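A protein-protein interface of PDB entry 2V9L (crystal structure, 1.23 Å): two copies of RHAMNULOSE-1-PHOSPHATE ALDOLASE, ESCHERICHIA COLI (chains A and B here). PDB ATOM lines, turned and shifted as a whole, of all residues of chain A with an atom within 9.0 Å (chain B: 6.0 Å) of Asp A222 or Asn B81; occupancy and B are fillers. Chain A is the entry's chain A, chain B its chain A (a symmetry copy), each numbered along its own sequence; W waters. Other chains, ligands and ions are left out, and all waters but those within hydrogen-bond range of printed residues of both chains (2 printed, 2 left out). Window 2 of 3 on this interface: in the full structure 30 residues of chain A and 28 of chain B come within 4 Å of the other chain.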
ATOM      1  N   TRP A   8     -26.518   6.364  11.500  1.00  0.00           N
ATOM      2  CA  TRP A   8     -26.472   7.033  10.211  1.00  0.00           C
ATOM      3  C   TRP A   8     -27.647   7.940   9.999  1.00  0.00           C
ATOM      4  O   TRP A   8     -27.531   9.016   9.391  1.00  0.00           O
ATOM      5  CB  TRP A   8     -26.392   6.002   9.080  1.00  0.00           C
ATOM      6  CG  TRP A   8     -27.608   5.177   8.780  1.00  0.00           C
ATOM      7  CD1 TRP A   8     -27.839   3.887   9.232  1.00  0.00           C
ATOM      8  CD2 TRP A   8     -28.735   5.553   7.992  1.00  0.00           C
ATOM      9  NE1 TRP A   8     -29.046   3.480   8.746  1.00  0.00           N
ATOM     10  CE2 TRP A   8     -29.633   4.472   7.980  1.00  0.00           C
ATOM     11  CE3 TRP A   8     -29.077   6.717   7.277  1.00  0.00           C
ATOM     12  CZ2 TRP A   8     -30.844   4.513   7.292  1.00  0.00           C
ATOM     13  CZ3 TRP A   8     -30.282   6.760   6.602  1.00  0.00           C
ATOM     14  CH2 TRP A   8     -31.155   5.670   6.612  1.00  0.00           C
ATOM     15  N   GLN A  11     -27.574  11.107  12.351  1.00  0.00           N
ATOM     16  CA  GLN A  11     -26.536  11.988  11.783  1.00  0.00           C
ATOM     17  C   GLN A  11     -26.985  12.599  10.469  1.00  0.00           C
ATOM     18  O   GLN A  11     -26.701  13.773  10.217  1.00  0.00           O
ATOM     19  CB  GLN A  11     -25.199  11.259  11.669  1.00  0.00           C
ATOM     20  CG  GLN A  11     -24.553  10.930  13.013  1.00  0.00           C
ATOM     21  CD  GLN A  11     -24.087  12.192  13.735  1.00  0.00           C
ATOM     22  OE1 GLN A  11     -23.350  13.013  13.146  1.00  0.00           O
ATOM     23  NE2 GLN A  11     -24.480  12.411  14.972  1.00  0.00           N
ATOM     24  N   GLY A  12     -27.652  11.809   9.634  1.00  0.00           N
ATOM     25  CA  GLY A  12     -28.140  12.338   8.388  1.00  0.00           C
ATOM     26  C   GLY A  12     -29.203  13.392   8.525  1.00  0.00           C
ATOM     27  O   GLY A  12     -29.231  14.384   7.790  1.00  0.00           O
ATOM     28  N   MET A  13     -30.111  13.205   9.507  1.00  0.00           N
ATOM     29  CA  MET A  13     -31.113  14.231   9.789  1.00  0.00           C
ATOM     30  C   MET A  13     -30.415  15.501  10.285  1.00  0.00           C
ATOM     31  O   MET A  13     -30.853  16.609   9.892  1.00  0.00           O
ATOM     32  CB  MET A  13     -32.103  13.715  10.814  1.00  0.00           C
ATOM     33  CG  MET A  13     -33.016  12.625  10.337  1.00  0.00           C
ATOM     34  SD  MET A  13     -34.259  13.127   9.119  1.00  0.00           S
ATOM     35  CE  MET A  13     -35.400  14.032  10.181  1.00  0.00           C
ATOM     36  N   LYS A  15     -27.398  16.498   9.464  1.00  0.00           N
ATOM     37  CA  LYS A  15     -26.694  17.132   8.349  1.00  0.00           C
ATOM     38  C   LYS A  15     -27.687  17.883   7.461  1.00  0.00           C
ATOM     39  O   LYS A  15     -27.430  19.027   7.057  1.00  0.00           O
ATOM     40  CB  LYS A  15     -25.948  16.058   7.523  1.00  0.00           C
ATOM     41  CG  LYS A  15     -25.056  16.650   6.485  1.00  0.00           C
ATOM     42  CD  LYS A  15     -24.383  15.638   5.580  1.00  0.00           C
ATOM     43  CE  LYS A  15     -24.964  15.552   4.257  1.00  0.00           C
ATOM     44  NZ  LYS A  15     -24.463  14.442   3.403  1.00  0.00           N
ATOM     45  N   ALA A  16     -28.832  17.240   7.093  1.00  0.00           N
ATOM     46  CA  ALA A  16     -29.729  17.879   6.186  1.00  0.00           C
ATOM     47  C   ALA A  16     -30.372  19.125   6.780  1.00  0.00           C
ATOM     48  O   ALA A  16     -30.494  20.143   6.097  1.00  0.00           O
ATOM     49  CB  ALA A  16     -30.804  16.858   5.773  1.00  0.00           C
ATOM     50  N   ASP A  19     -27.638  21.872   7.093  1.00  0.00           N
ATOM     51  CA  ASP A  19     -27.298  22.425   5.793  1.00  0.00           C
ATOM     52  C   ASP A  19     -28.408  23.339   5.294  1.00  0.00           C
ATOM     53  O   ASP A  19     -28.143  24.418   4.739  1.00  0.00           O
ATOM     54  CB  ASP A  19     -27.043  21.307   4.776  1.00  0.00           C
ATOM     55  CG  ASP A  19     -25.753  20.543   4.966  1.00  0.00           C
ATOM     56  OD1 ASP A  19     -24.878  21.007   5.741  1.00  0.00           O
ATOM     57  OD2 ASP A  19     -25.622  19.495   4.307  1.00  0.00           O
ATOM     58  N   LEU A  33     -39.013  17.624   7.924  1.00  0.00           N
ATOM     59  CA  LEU A  33     -38.280  16.569   7.293  1.00  0.00           C
ATOM     60  C   LEU A  33     -38.676  15.244   7.929  1.00  0.00           C
ATOM     61  O   LEU A  33     -38.641  15.114   9.139  1.00  0.00           O
ATOM     62  CB  LEU A  33     -36.779  16.824   7.461  1.00  0.00           C
ATOM     63  CG  LEU A  33     -35.832  15.820   6.823  1.00  0.00           C
ATOM     64  CD1 LEU A  33     -36.013  15.748   5.310  1.00  0.00           C
ATOM     65  CD2 LEU A  33     -34.383  16.207   7.160  1.00  0.00           C
ATOM     66  N   LEU A  35     -38.077  10.875   7.279  1.00  0.00           N
ATOM     67  CA  LEU A  35     -37.336   9.820   6.631  1.00  0.00           C
ATOM     68  C   LEU A  35     -37.892   8.457   7.058  1.00  0.00           C
ATOM     69  O   LEU A  35     -37.936   8.158   8.276  1.00  0.00           O
ATOM     70  CB  LEU A  35     -35.836   9.938   7.041  1.00  0.00           C
ATOM     71  CG  LEU A  35     -34.922   8.757   6.780  1.00  0.00           C
ATOM     72  CD1 LEU A  35     -34.780   8.423   5.295  1.00  0.00           C
ATOM     73  CD2 LEU A  35     -33.565   9.007   7.390  1.00  0.00           C
ATOM     74  N   VAL A 138     -37.963   9.785   1.598  1.00  0.00           N
ATOM     75  CA  VAL A 138     -37.796  11.073   2.255  1.00  0.00           C
ATOM     76  C   VAL A 138     -38.813  12.054   1.697  1.00  0.00           C
ATOM     77  O   VAL A 138     -39.001  12.139   0.488  1.00  0.00           O
ATOM     78  CB  VAL A 138     -36.372  11.635   2.000  1.00  0.00           C
ATOM     79  CG1 VAL A 138     -36.233  13.007   2.664  1.00  0.00           C
ATOM     80  CG2 VAL A 138     -35.338  10.665   2.538  1.00  0.00           C
ATOM     81  N   MET A 140     -39.145  16.224   2.253  1.00  0.00           N
ATOM     82  CA  MET A 140     -38.500  17.405   2.820  1.00  0.00           C
ATOM     83  C   MET A 140     -39.278  18.631   2.399  1.00  0.00           C
ATOM     84  O   MET A 140     -39.550  18.823   1.214  1.00  0.00           O
ATOM     85  CB  MET A 140     -37.047  17.542   2.316  1.00  0.00           C
ATOM     86  CG  MET A 140     -36.356  18.764   2.896  1.00  0.00           C
ATOM     87  SD  MET A 140     -34.580  18.699   2.538  1.00  0.00           S
ATOM     88  CE  MET A 140     -34.179  20.461   2.747  1.00  0.00           C
ATOM     89  N   VAL A 175     -32.559  16.184 -13.501  1.00  0.00           N
ATOM     90  CA  VAL A 175     -32.821  15.984 -12.084  1.00  0.00           C
ATOM     91  C   VAL A 175     -34.316  15.836 -11.758  1.00  0.00           C
ATOM     92  O   VAL A 175     -34.694  15.014 -10.915  1.00  0.00           O
ATOM     93  CB  VAL A 175     -32.137  17.076 -11.260  1.00  0.00           C
ATOM     94  CG1 VAL A 175     -32.444  16.948  -9.784  1.00  0.00           C
ATOM     95  CG2 VAL A 175     -30.632  17.023 -11.446  1.00  0.00           C
ATOM     96  N   SER A 217     -39.365  14.918  -2.702  1.00  0.00           N
ATOM     97  CA  SER A 217     -39.287  13.519  -2.328  1.00  0.00           C
ATOM     98  C   SER A 217     -38.116  12.833  -3.045  1.00  0.00           C
ATOM     99  O   SER A 217     -37.811  13.170  -4.194  1.00  0.00           O
ATOM    100  CB  SER A 217     -40.577  12.793  -2.749  1.00  0.00           C
ATOM    101  OG  SER A 217     -40.610  11.437  -2.363  1.00  0.00           O
ATOM    102  N   GLY A 218     -37.503  11.865  -2.402  1.00  0.00           N
ATOM    103  CA  GLY A 218     -36.439  11.107  -3.026  1.00  0.00           C
ATOM    104  C   GLY A 218     -36.038   9.906  -2.210  1.00  0.00           C
ATOM    105  O   GLY A 218     -36.602   9.675  -1.115  1.00  0.00           O
ATOM    106  N   PRO A 219     -35.120   9.085  -2.705  1.00  0.00           N
ATOM    107  CA  PRO A 219     -34.769   7.832  -2.018  1.00  0.00           C
ATOM    108  C   PRO A 219     -33.888   7.954  -0.777  1.00  0.00           C
ATOM    109  O   PRO A 219     -33.884   7.052   0.084  1.00  0.00           O
ATOM    110  CB  PRO A 219     -34.050   7.023  -3.117  1.00  0.00           C
ATOM    111  CG  PRO A 219     -33.656   7.996  -4.126  1.00  0.00           C
ATOM    112  CD  PRO A 219     -34.527   9.174  -4.048  1.00  0.00           C
ATOM    113  N   THR A 220     -33.107   9.048  -0.705  1.00  0.00           N
ATOM    114  CA  THR A 220     -32.170   9.263   0.337  1.00  0.00           C
ATOM    115  C   THR A 220     -32.205  10.734   0.753  1.00  0.00           C
ATOM    116  O   THR A 220     -32.693  11.577  -0.023  1.00  0.00           O
ATOM    117  CB  THR A 220     -30.701   8.919   0.029  1.00  0.00           C
ATOM    118  OG1 THR A 220     -30.265   9.832  -0.975  1.00  0.00           O
ATOM    119  CG2 THR A 220     -30.558   7.449  -0.408  1.00  0.00           C
ATOM    120  N   LEU A 221     -31.706  11.027   1.938  1.00  0.00           N
ATOM    121  CA  LEU A 221     -31.623  12.420   2.378  1.00  0.00           C
ATOM    122  C   LEU A 221     -30.819  13.251   1.385  1.00  0.00           C
ATOM    123  O   LEU A 221     -31.275  14.345   0.973  1.00  0.00           O
ATOM    124  CB  LEU A 221     -30.989  12.451   3.768  1.00  0.00           C
ATOM    125  CG  LEU A 221     -31.873  11.955   4.920  1.00  0.00           C
ATOM    126  CD1 LEU A 221     -31.020  11.728   6.168  1.00  0.00           C
ATOM    127  CD2 LEU A 221     -33.024  12.924   5.196  1.00  0.00           C
ATOM    128  N   ASP A 222     -29.642  12.790   0.985  1.00  0.00           N
ATOM    129  CA  ASP A 222     -28.836  13.602   0.069  1.00  0.00           C
ATOM    130  C   ASP A 222     -29.524  13.777  -1.262  1.00  0.00           C
ATOM    131  O   ASP A 222     -29.449  14.855  -1.870  1.00  0.00           O
ATOM    132  CB  ASP A 222     -27.473  12.955  -0.161  1.00  0.00           C
ATOM    133  CG  ASP A 222     -26.453  13.271   0.851  1.00  0.00           C
ATOM    134  OD1 ASP A 222     -25.381  12.613   0.869  1.00  0.00           O
ATOM    135  OD2 ASP A 222     -26.623  14.240   1.610  1.00  0.00           O
ATOM    136  N   GLU A 223     -30.156  12.723  -1.812  1.00  0.00           N
ATOM    137  CA  GLU A 223     -30.788  12.903  -3.092  1.00  0.00           C
ATOM    138  C   GLU A 223     -31.948  13.888  -3.017  1.00  0.00           C
ATOM    139  O   GLU A 223     -32.212  14.640  -3.952  1.00  0.00           O
ATOM    140  CB  GLU A 223     -31.238  11.553  -3.704  1.00  0.00           C
ATOM    141  CG  GLU A 223     -30.115  10.648  -4.152  1.00  0.00           C
ATOM    142  CD  GLU A 223     -30.413   9.184  -4.367  1.00  0.00           C
ATOM    143  OE1 GLU A 223     -30.299   8.694  -5.496  1.00  0.00           O
ATOM    144  OE2 GLU A 223     -30.751   8.462  -3.402  1.00  0.00           O
ATOM    145  N   THR A 224     -32.674  13.867  -1.901  1.00  0.00           N
ATOM    146  CA  THR A 224     -33.831  14.770  -1.752  1.00  0.00           C
ATOM    147  C   THR A 224     -33.391  16.210  -1.527  1.00  0.00           C
ATOM    148  O   THR A 224     -33.905  17.160  -2.119  1.00  0.00           O
ATOM    149  CB  THR A 224     -34.734  14.274  -0.600  1.00  0.00           C
ATOM    150  OG1 THR A 224     -35.042  12.880  -0.820  1.00  0.00           O
ATOM    151  CG2 THR A 224     -36.038  15.027  -0.594  1.00  0.00           C
ATOM    152  N   PHE A 225     -32.390  16.372  -0.624  1.00  0.00           N
ATOM    153  CA  PHE A 225     -31.797  17.696  -0.444  1.00  0.00           C
ATOM    154  C   PHE A 225     -31.282  18.219  -1.784  1.00  0.00           C
ATOM    155  O   PHE A 225     -31.497  19.371  -2.123  1.00  0.00           O
ATOM    156  CB  PHE A 225     -30.686  17.605   0.610  1.00  0.00           C
ATOM    157  CG  PHE A 225     -30.103  18.947   0.962  1.00  0.00           C
ATOM    158  CD1 PHE A 225     -30.491  19.590   2.122  1.00  0.00           C
ATOM    159  CD2 PHE A 225     -29.177  19.570   0.171  1.00  0.00           C
ATOM    160  CE1 PHE A 225     -29.951  20.826   2.427  1.00  0.00           C
ATOM    161  CE2 PHE A 225     -28.686  20.808   0.476  1.00  0.00           C
ATOM    162  CZ  PHE A 225     -29.078  21.458   1.605  1.00  0.00           C
ATOM    163  N   GLY A 226     -30.541  17.369  -2.503  1.00  0.00           N
ATOM    164  CA  GLY A 226     -29.962  17.790  -3.759  1.00  0.00           C
ATOM    165  C   GLY A 226     -30.994  18.135  -4.799  1.00  0.00           C
ATOM    166  O   GLY A 226     -30.719  19.018  -5.628  1.00  0.00           O
ATOM    167  N   LEU A 227     -32.124  17.460  -4.799  1.00  0.00           N
ATOM    168  CA  LEU A 227     -33.250  17.807  -5.687  1.00  0.00           C
ATOM    169  C   LEU A 227     -33.711  19.212  -5.426  1.00  0.00           C
ATOM    170  O   LEU A 227     -33.879  20.052  -6.316  1.00  0.00           O
ATOM    171  CB  LEU A 227     -34.361  16.782  -5.450  1.00  0.00           C
ATOM    172  CG  LEU A 227     -35.709  17.053  -6.070  1.00  0.00           C
ATOM    173  CD1 LEU A 227     -35.671  16.997  -7.602  1.00  0.00           C
ATOM    174  CD2 LEU A 227     -36.734  16.068  -5.509  1.00  0.00           C
ATOM    175  N   ILE A 228     -34.007  19.516  -4.156  1.00  0.00           N
ATOM    176  CA  ILE A 228     -34.436  20.872  -3.782  1.00  0.00           C
ATOM    177  C   ILE A 228     -33.341  21.888  -4.054  1.00  0.00           C
ATOM    178  O   ILE A 228     -33.644  22.969  -4.592  1.00  0.00           O
ATOM    179  CB  ILE A 228     -34.886  20.911  -2.308  1.00  0.00           C
ATOM    180  CG1 ILE A 228     -36.157  20.088  -2.119  1.00  0.00           C
ATOM    181  CG2 ILE A 228     -35.045  22.348  -1.818  1.00  0.00           C
ATOM    182  CD1 ILE A 228     -36.560  19.889  -0.667  1.00  0.00           C
ATOM    183  N   ASP A 229     -32.102  21.572  -3.713  1.00  0.00           N
ATOM    184  CA  ASP A 229     -30.993  22.499  -3.934  1.00  0.00           C
ATOM    185  C   ASP A 229     -30.878  22.841  -5.417  1.00  0.00           C
ATOM    186  O   ASP A 229     -30.567  23.984  -5.790  1.00  0.00           O
ATOM    187  CB  ASP A 229     -29.716  21.919  -3.361  1.00  0.00           C
ATOM    188  CG  ASP A 229     -28.597  22.906  -3.021  1.00  0.00           C
ATOM    189  OD1 ASP A 229     -28.891  24.087  -2.814  1.00  0.00           O
ATOM    190  OD2 ASP A 229     -27.438  22.436  -2.905  1.00  0.00           O
ATOM    191  N   THR A 230     -31.076  21.853  -6.284  1.00  0.00           N
ATOM    192  CA  THR A 230     -31.010  22.073  -7.729  1.00  0.00           C
ATOM    193  C   THR A 230     -32.087  23.048  -8.190  1.00  0.00           C
ATOM    194  O   THR A 230     -31.837  24.026  -8.913  1.00  0.00           O
ATOM    195  CB  THR A 230     -31.076  20.740  -8.483  1.00  0.00           C
ATOM    196  OG1 THR A 230     -29.956  19.940  -8.152  1.00  0.00           O
ATOM    197  CG2 THR A 230     -31.120  20.989  -9.949  1.00  0.00           C
ATOM    198  N   ARG B  28     -25.926  19.546  -5.425  1.00  0.00           N
ATOM    199  CA  ARG B  28     -26.030  18.143  -5.845  1.00  0.00           C
ATOM    200  C   ARG B  28     -24.660  17.638  -6.291  1.00  0.00           C
ATOM    201  O   ARG B  28     -23.657  17.825  -5.592  1.00  0.00           O
ATOM    202  CB  ARG B  28     -27.172  17.969  -6.848  1.00  0.00           C
ATOM    203  CG  ARG B  28     -27.742  16.578  -7.016  1.00  0.00           C
ATOM    204  CD  ARG B  28     -28.759  16.532  -8.113  1.00  0.00           C
ATOM    205  NE  ARG B  28     -29.431  15.263  -8.343  1.00  0.00           N
ATOM    206  CZ  ARG B  28     -29.099  14.447  -9.341  1.00  0.00           C
ATOM    207  NH1 ARG B  28     -28.079  14.602 -10.156  1.00  0.00           N
ATOM    208  NH2 ARG B  28     -29.851  13.365  -9.515  1.00  0.00           N
ATOM    209  N   PHE B  78     -21.225  14.350  -4.484  1.00  0.00           N
ATOM    210  CA  PHE B  78     -21.486  15.705  -4.069  1.00  0.00           C
ATOM    211  C   PHE B  78     -20.227  16.369  -3.501  1.00  0.00           C
ATOM    212  O   PHE B  78     -19.584  15.817  -2.584  1.00  0.00           O
ATOM    213  CB  PHE B  78     -22.537  15.724  -2.934  1.00  0.00           C
ATOM    214  CG  PHE B  78     -23.950  15.389  -3.318  1.00  0.00           C
ATOM    215  CD1 PHE B  78     -24.319  14.782  -4.531  1.00  0.00           C
ATOM    216  CD2 PHE B  78     -24.967  15.721  -2.421  1.00  0.00           C
ATOM    217  CE1 PHE B  78     -25.668  14.536  -4.767  1.00  0.00           C
ATOM    218  CE2 PHE B  78     -26.281  15.446  -2.652  1.00  0.00           C
ATOM    219  CZ  PHE B  78     -26.617  14.823  -3.822  1.00  0.00           C
ATOM    220  N   PHE B  79     -19.887  17.575  -3.984  1.00  0.00           N
ATOM    221  CA  PHE B  79     -18.770  18.297  -3.386  1.00  0.00           C
ATOM    222  C   PHE B  79     -18.949  18.443  -1.880  1.00  0.00           C
ATOM    223  O   PHE B  79     -17.984  18.375  -1.140  1.00  0.00           O
ATOM    224  CB  PHE B  79     -18.622  19.713  -3.993  1.00  0.00           C
ATOM    225  CG  PHE B  79     -17.835  19.787  -5.275  1.00  0.00           C
ATOM    226  CD1 PHE B  79     -17.623  18.690  -6.116  1.00  0.00           C
ATOM    227  CD2 PHE B  79     -17.286  21.006  -5.635  1.00  0.00           C
ATOM    228  CE1 PHE B  79     -16.891  18.856  -7.280  1.00  0.00           C
ATOM    229  CE2 PHE B  79     -16.564  21.170  -6.797  1.00  0.00           C
ATOM    230  CZ  PHE B  79     -16.352  20.077  -7.622  1.00  0.00           C
ATOM    231  N   ARG B  80     -20.194  18.622  -1.404  1.00  0.00           N
ATOM    232  CA  ARG B  80     -20.437  18.776   0.034  1.00  0.00           C
ATOM    233  C   ARG B  80     -19.924  17.611   0.864  1.00  0.00           C
ATOM    234  O   ARG B  80     -19.595  17.790   2.031  1.00  0.00           O
ATOM    235  CB  ARG B  80     -21.951  18.956   0.264  1.00  0.00           C
ATOM    236  CG  ARG B  80     -22.326  19.336   1.698  1.00  0.00           C
ATOM    237  CD  ARG B  80     -22.713  18.153   2.546  1.00  0.00           C
ATOM    238  NE  ARG B  80     -23.010  18.643   3.898  1.00  0.00           N
ATOM    239  CZ  ARG B  80     -22.062  18.845   4.792  1.00  0.00           C
ATOM    240  NH1 ARG B  80     -20.789  18.556   4.632  1.00  0.00           N
ATOM    241  NH2 ARG B  80     -22.428  19.351   5.926  1.00  0.00           N
ATOM    242  N   ASN B  81     -19.916  16.412   0.292  1.00  0.00           N
ATOM    243  CA  ASN B  81     -19.580  15.198   1.008  1.00  0.00           C
ATOM    244  C   ASN B  81     -18.100  14.815   0.980  1.00  0.00           C
ATOM    245  O   ASN B  81     -17.707  13.903   1.706  1.00  0.00           O
ATOM    246  CB  ASN B  81     -20.396  14.019   0.477  1.00  0.00           C
ATOM    247  CG  ASN B  81     -21.865  14.140   0.862  1.00  0.00           C
ATOM    248  OD1 ASN B  81     -22.215  14.779   1.843  1.00  0.00           O
ATOM    249  ND2 ASN B  81     -22.696  13.460   0.085  1.00  0.00           N
ATOM    250  N   VAL B  82     -17.311  15.485   0.147  1.00  0.00           N
ATOM    251  CA  VAL B  82     -15.900  15.098  -0.008  1.00  0.00           C
ATOM    252  C   VAL B  82     -15.203  15.112   1.337  1.00  0.00           C
ATOM    253  O   VAL B  82     -14.459  14.182   1.700  1.00  0.00           O
ATOM    254  CB  VAL B  82     -15.196  15.971  -1.054  1.00  0.00           C
ATOM    255  CG1 VAL B  82     -13.693  15.694  -1.063  1.00  0.00           C
ATOM    256  CG2 VAL B  82     -15.808  15.765  -2.425  1.00  0.00           C
ATOM    257  N   GLN B  83     -15.433  16.169   2.150  1.00  0.00           N
ATOM    258  CA  GLN B  83     -14.812  16.250   3.452  1.00  0.00           C
ATOM    259  C   GLN B  83     -15.235  15.163   4.411  1.00  0.00           C
ATOM    260  O   GLN B  83     -14.514  14.857   5.356  1.00  0.00           O
ATOM    261  CB  GLN B  83     -15.142  17.633   4.052  1.00  0.00           C
ATOM    262  CG  GLN B  83     -16.630  17.795   4.378  1.00  0.00           C
ATOM    263  CD  GLN B  83     -16.975  19.223   4.773  1.00  0.00           C
ATOM    264  OE1 GLN B  83     -16.374  19.703   5.774  1.00  0.00           O
ATOM    265  NE2 GLN B  83     -17.882  19.810   4.018  1.00  0.00           N
ATOM    266  N   LEU B  84     -16.425  14.619   4.229  1.00  0.00           N
ATOM    267  CA  LEU B  84     -16.990  13.616   5.131  1.00  0.00           C
ATOM    268  C   LEU B  84     -16.436  12.229   4.807  1.00  0.00           C
ATOM    269  O   LEU B  84     -16.346  11.412   5.736  1.00  0.00           O
ATOM    270  CB  LEU B  84     -18.486  13.625   5.090  1.00  0.00           C
ATOM    271  CG  LEU B  84     -19.191  14.927   5.369  1.00  0.00           C
ATOM    272  CD1 LEU B  84     -20.705  14.766   5.238  1.00  0.00           C
ATOM    273  CD2 LEU B  84     -18.836  15.457   6.763  1.00  0.00           C
ATOM    274  N   ASP B  85     -16.112  11.950   3.565  1.00  0.00           N
ATOM    275  CA  ASP B  85     -15.689  10.619   3.152  1.00  0.00           C
ATOM    276  C   ASP B  85     -14.868  10.764   1.865  1.00  0.00           C
ATOM    277  O   ASP B  85     -15.384  10.548   0.785  1.00  0.00           O
ATOM    278  CB  ASP B  85     -16.840   9.654   2.988  1.00  0.00           C
ATOM    279  CG  ASP B  85     -16.460   8.191   2.883  1.00  0.00           C
ATOM    280  OD1 ASP B  85     -17.397   7.365   3.070  1.00  0.00           O
ATOM    281  OD2 ASP B  85     -15.253   7.936   2.634  1.00  0.00           O
ATOM    282  N   PRO B  86     -13.590  11.161   2.019  1.00  0.00           N
ATOM    283  CA  PRO B  86     -12.787  11.368   0.833  1.00  0.00           C
ATOM    284  C   PRO B  86     -12.699  10.153  -0.047  1.00  0.00           C
ATOM    285  O   PRO B  86     -12.804  10.274  -1.293  1.00  0.00           O
ATOM    286  CB  PRO B  86     -11.460  11.838   1.399  1.00  0.00           C
ATOM    287  CG  PRO B  86     -11.710  12.288   2.781  1.00  0.00           C
ATOM    288  CD  PRO B  86     -12.938  11.594   3.255  1.00  0.00           C
ATOM    289  N   ASN B  89     -15.736   9.615  -2.371  1.00  0.00           N
ATOM    290  CA  ASN B  89     -16.070  10.669  -3.320  1.00  0.00           C
ATOM    291  C   ASN B  89     -14.935  11.065  -4.292  1.00  0.00           C
ATOM    292  O   ASN B  89     -15.220  11.727  -5.287  1.00  0.00           O
ATOM    293  CB  ASN B  89     -16.543  11.895  -2.536  1.00  0.00           C
ATOM    294  CG  ASN B  89     -17.874  11.572  -1.855  1.00  0.00           C
ATOM    295  OD1 ASN B  89     -18.880  11.417  -2.523  1.00  0.00           O
ATOM    296  ND2 ASN B  89     -17.812  11.461  -0.528  1.00  0.00           N
HETATM  297  O   HOH W   1     -27.174  19.747  -2.935  1.00  0.00           O
HETATM  298  O   HOH W   2     -31.590  14.552  -6.647  1.00  0.00           O
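No position is printed for both chains. Of the 9 pairs that touch across the chains among the printed residues, none has its exchanged pair printed and touching as well.
Asp A222 touches just these residues of chain B: Phe B78 (3.3 Å) and Asn B81 (2.9 Å). Of chain A, only Lys A15 and Asp A222 come within 4 Å of Asn B81. Of the printed residues of chain B, Thr A230 touches Arg B28. Of the printed residues of chain A, Leu B84 touches Lys A15. The nearest residue of chain B that does not touch Asp A222 is Arg B80 (5.6 Å). The nearest residue of chain A that does not touch Asn B81 is Asp A19 (6.3 Å). The nearest printed residue of chain B that does not touch Gly A226 is Phe B78 (4.5 Å).
Arg B80 touches Lys A15. Lys A15 touches Leu B84 (CD to CD1, 3.8 Å). Val A175 touches Arg B28 (CG2 to CZ, 3.7 Å). Asp A222 touches Phe B78 (O to CE2, 3.3 Å). Arg B28 touches Gly A226. Arg B28 touches Thr A230.
Water W1 lies within hydrogen-bond range of OD2 of Asp A229 (2.7 Å) and N of Arg B28 (2.8 Å). Water W2 lies within hydrogen-bond range of the backbone carbonyl oxygen of Glu A223 (2.8 Å), the guanidinium group of Arg B28 (2.8 Å) and the backbone NH of Leu A227 (3.5 Å).
The guanidinium group (NE) of Arg B80 is in salt-bridge range of the side-chain carboxylate (OD2) of Asp A19 (2.8 Å). The side-chain amide nitrogen of Asn B81 is in hydrogen-bond range of the side-chain carboxylate of Asp A222, at 2.9 Å. The side-chain amide oxygen (OD1) of Asn B81 lies within hydrogen-bond range of the side-chain amino group (NZ) of Lys A15, at 2.8 Å.
The backbone carbonyl oxygen of Gly A226 sits at hydrogen-bond distance from the side-chain hydroxyl of Thr A230 (2.8 Å). The side-chain amino group (NZ) of Lys A15 is in salt-bridge range of the side-chain carboxylate (OD2) of Asp A222 (2.8 Å). The backbone carbonyl oxygen (O) of Asn B81 is in hydrogen-bond range of the side-chain amide nitrogen (ND2) of Asn B89 (3.3 Å). The side-chain amide nitrogen (NE2) of Gln B83 sits close to the guanidinium group (NH1) of Arg B80 (3.2 Å).
Of the 11 printed residues of chain B, 5 touch a printed residue of chain A. Printed residues of chain B that touch a printed residue of chain A: Arg B28, Phe B78, Arg B80, Asn B81 and Leu B84. Hydrophobic or aromatic side chains of chain A that line the printed part of chain B: Val A175. Among the printed residues, 9 pairs touch across the chains. Among the printed residues, Asp or Glu carboxylates within 4 Å of a Lys or Arg side-chain nitrogen of the other chain: Asp A19 with Arg B80.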
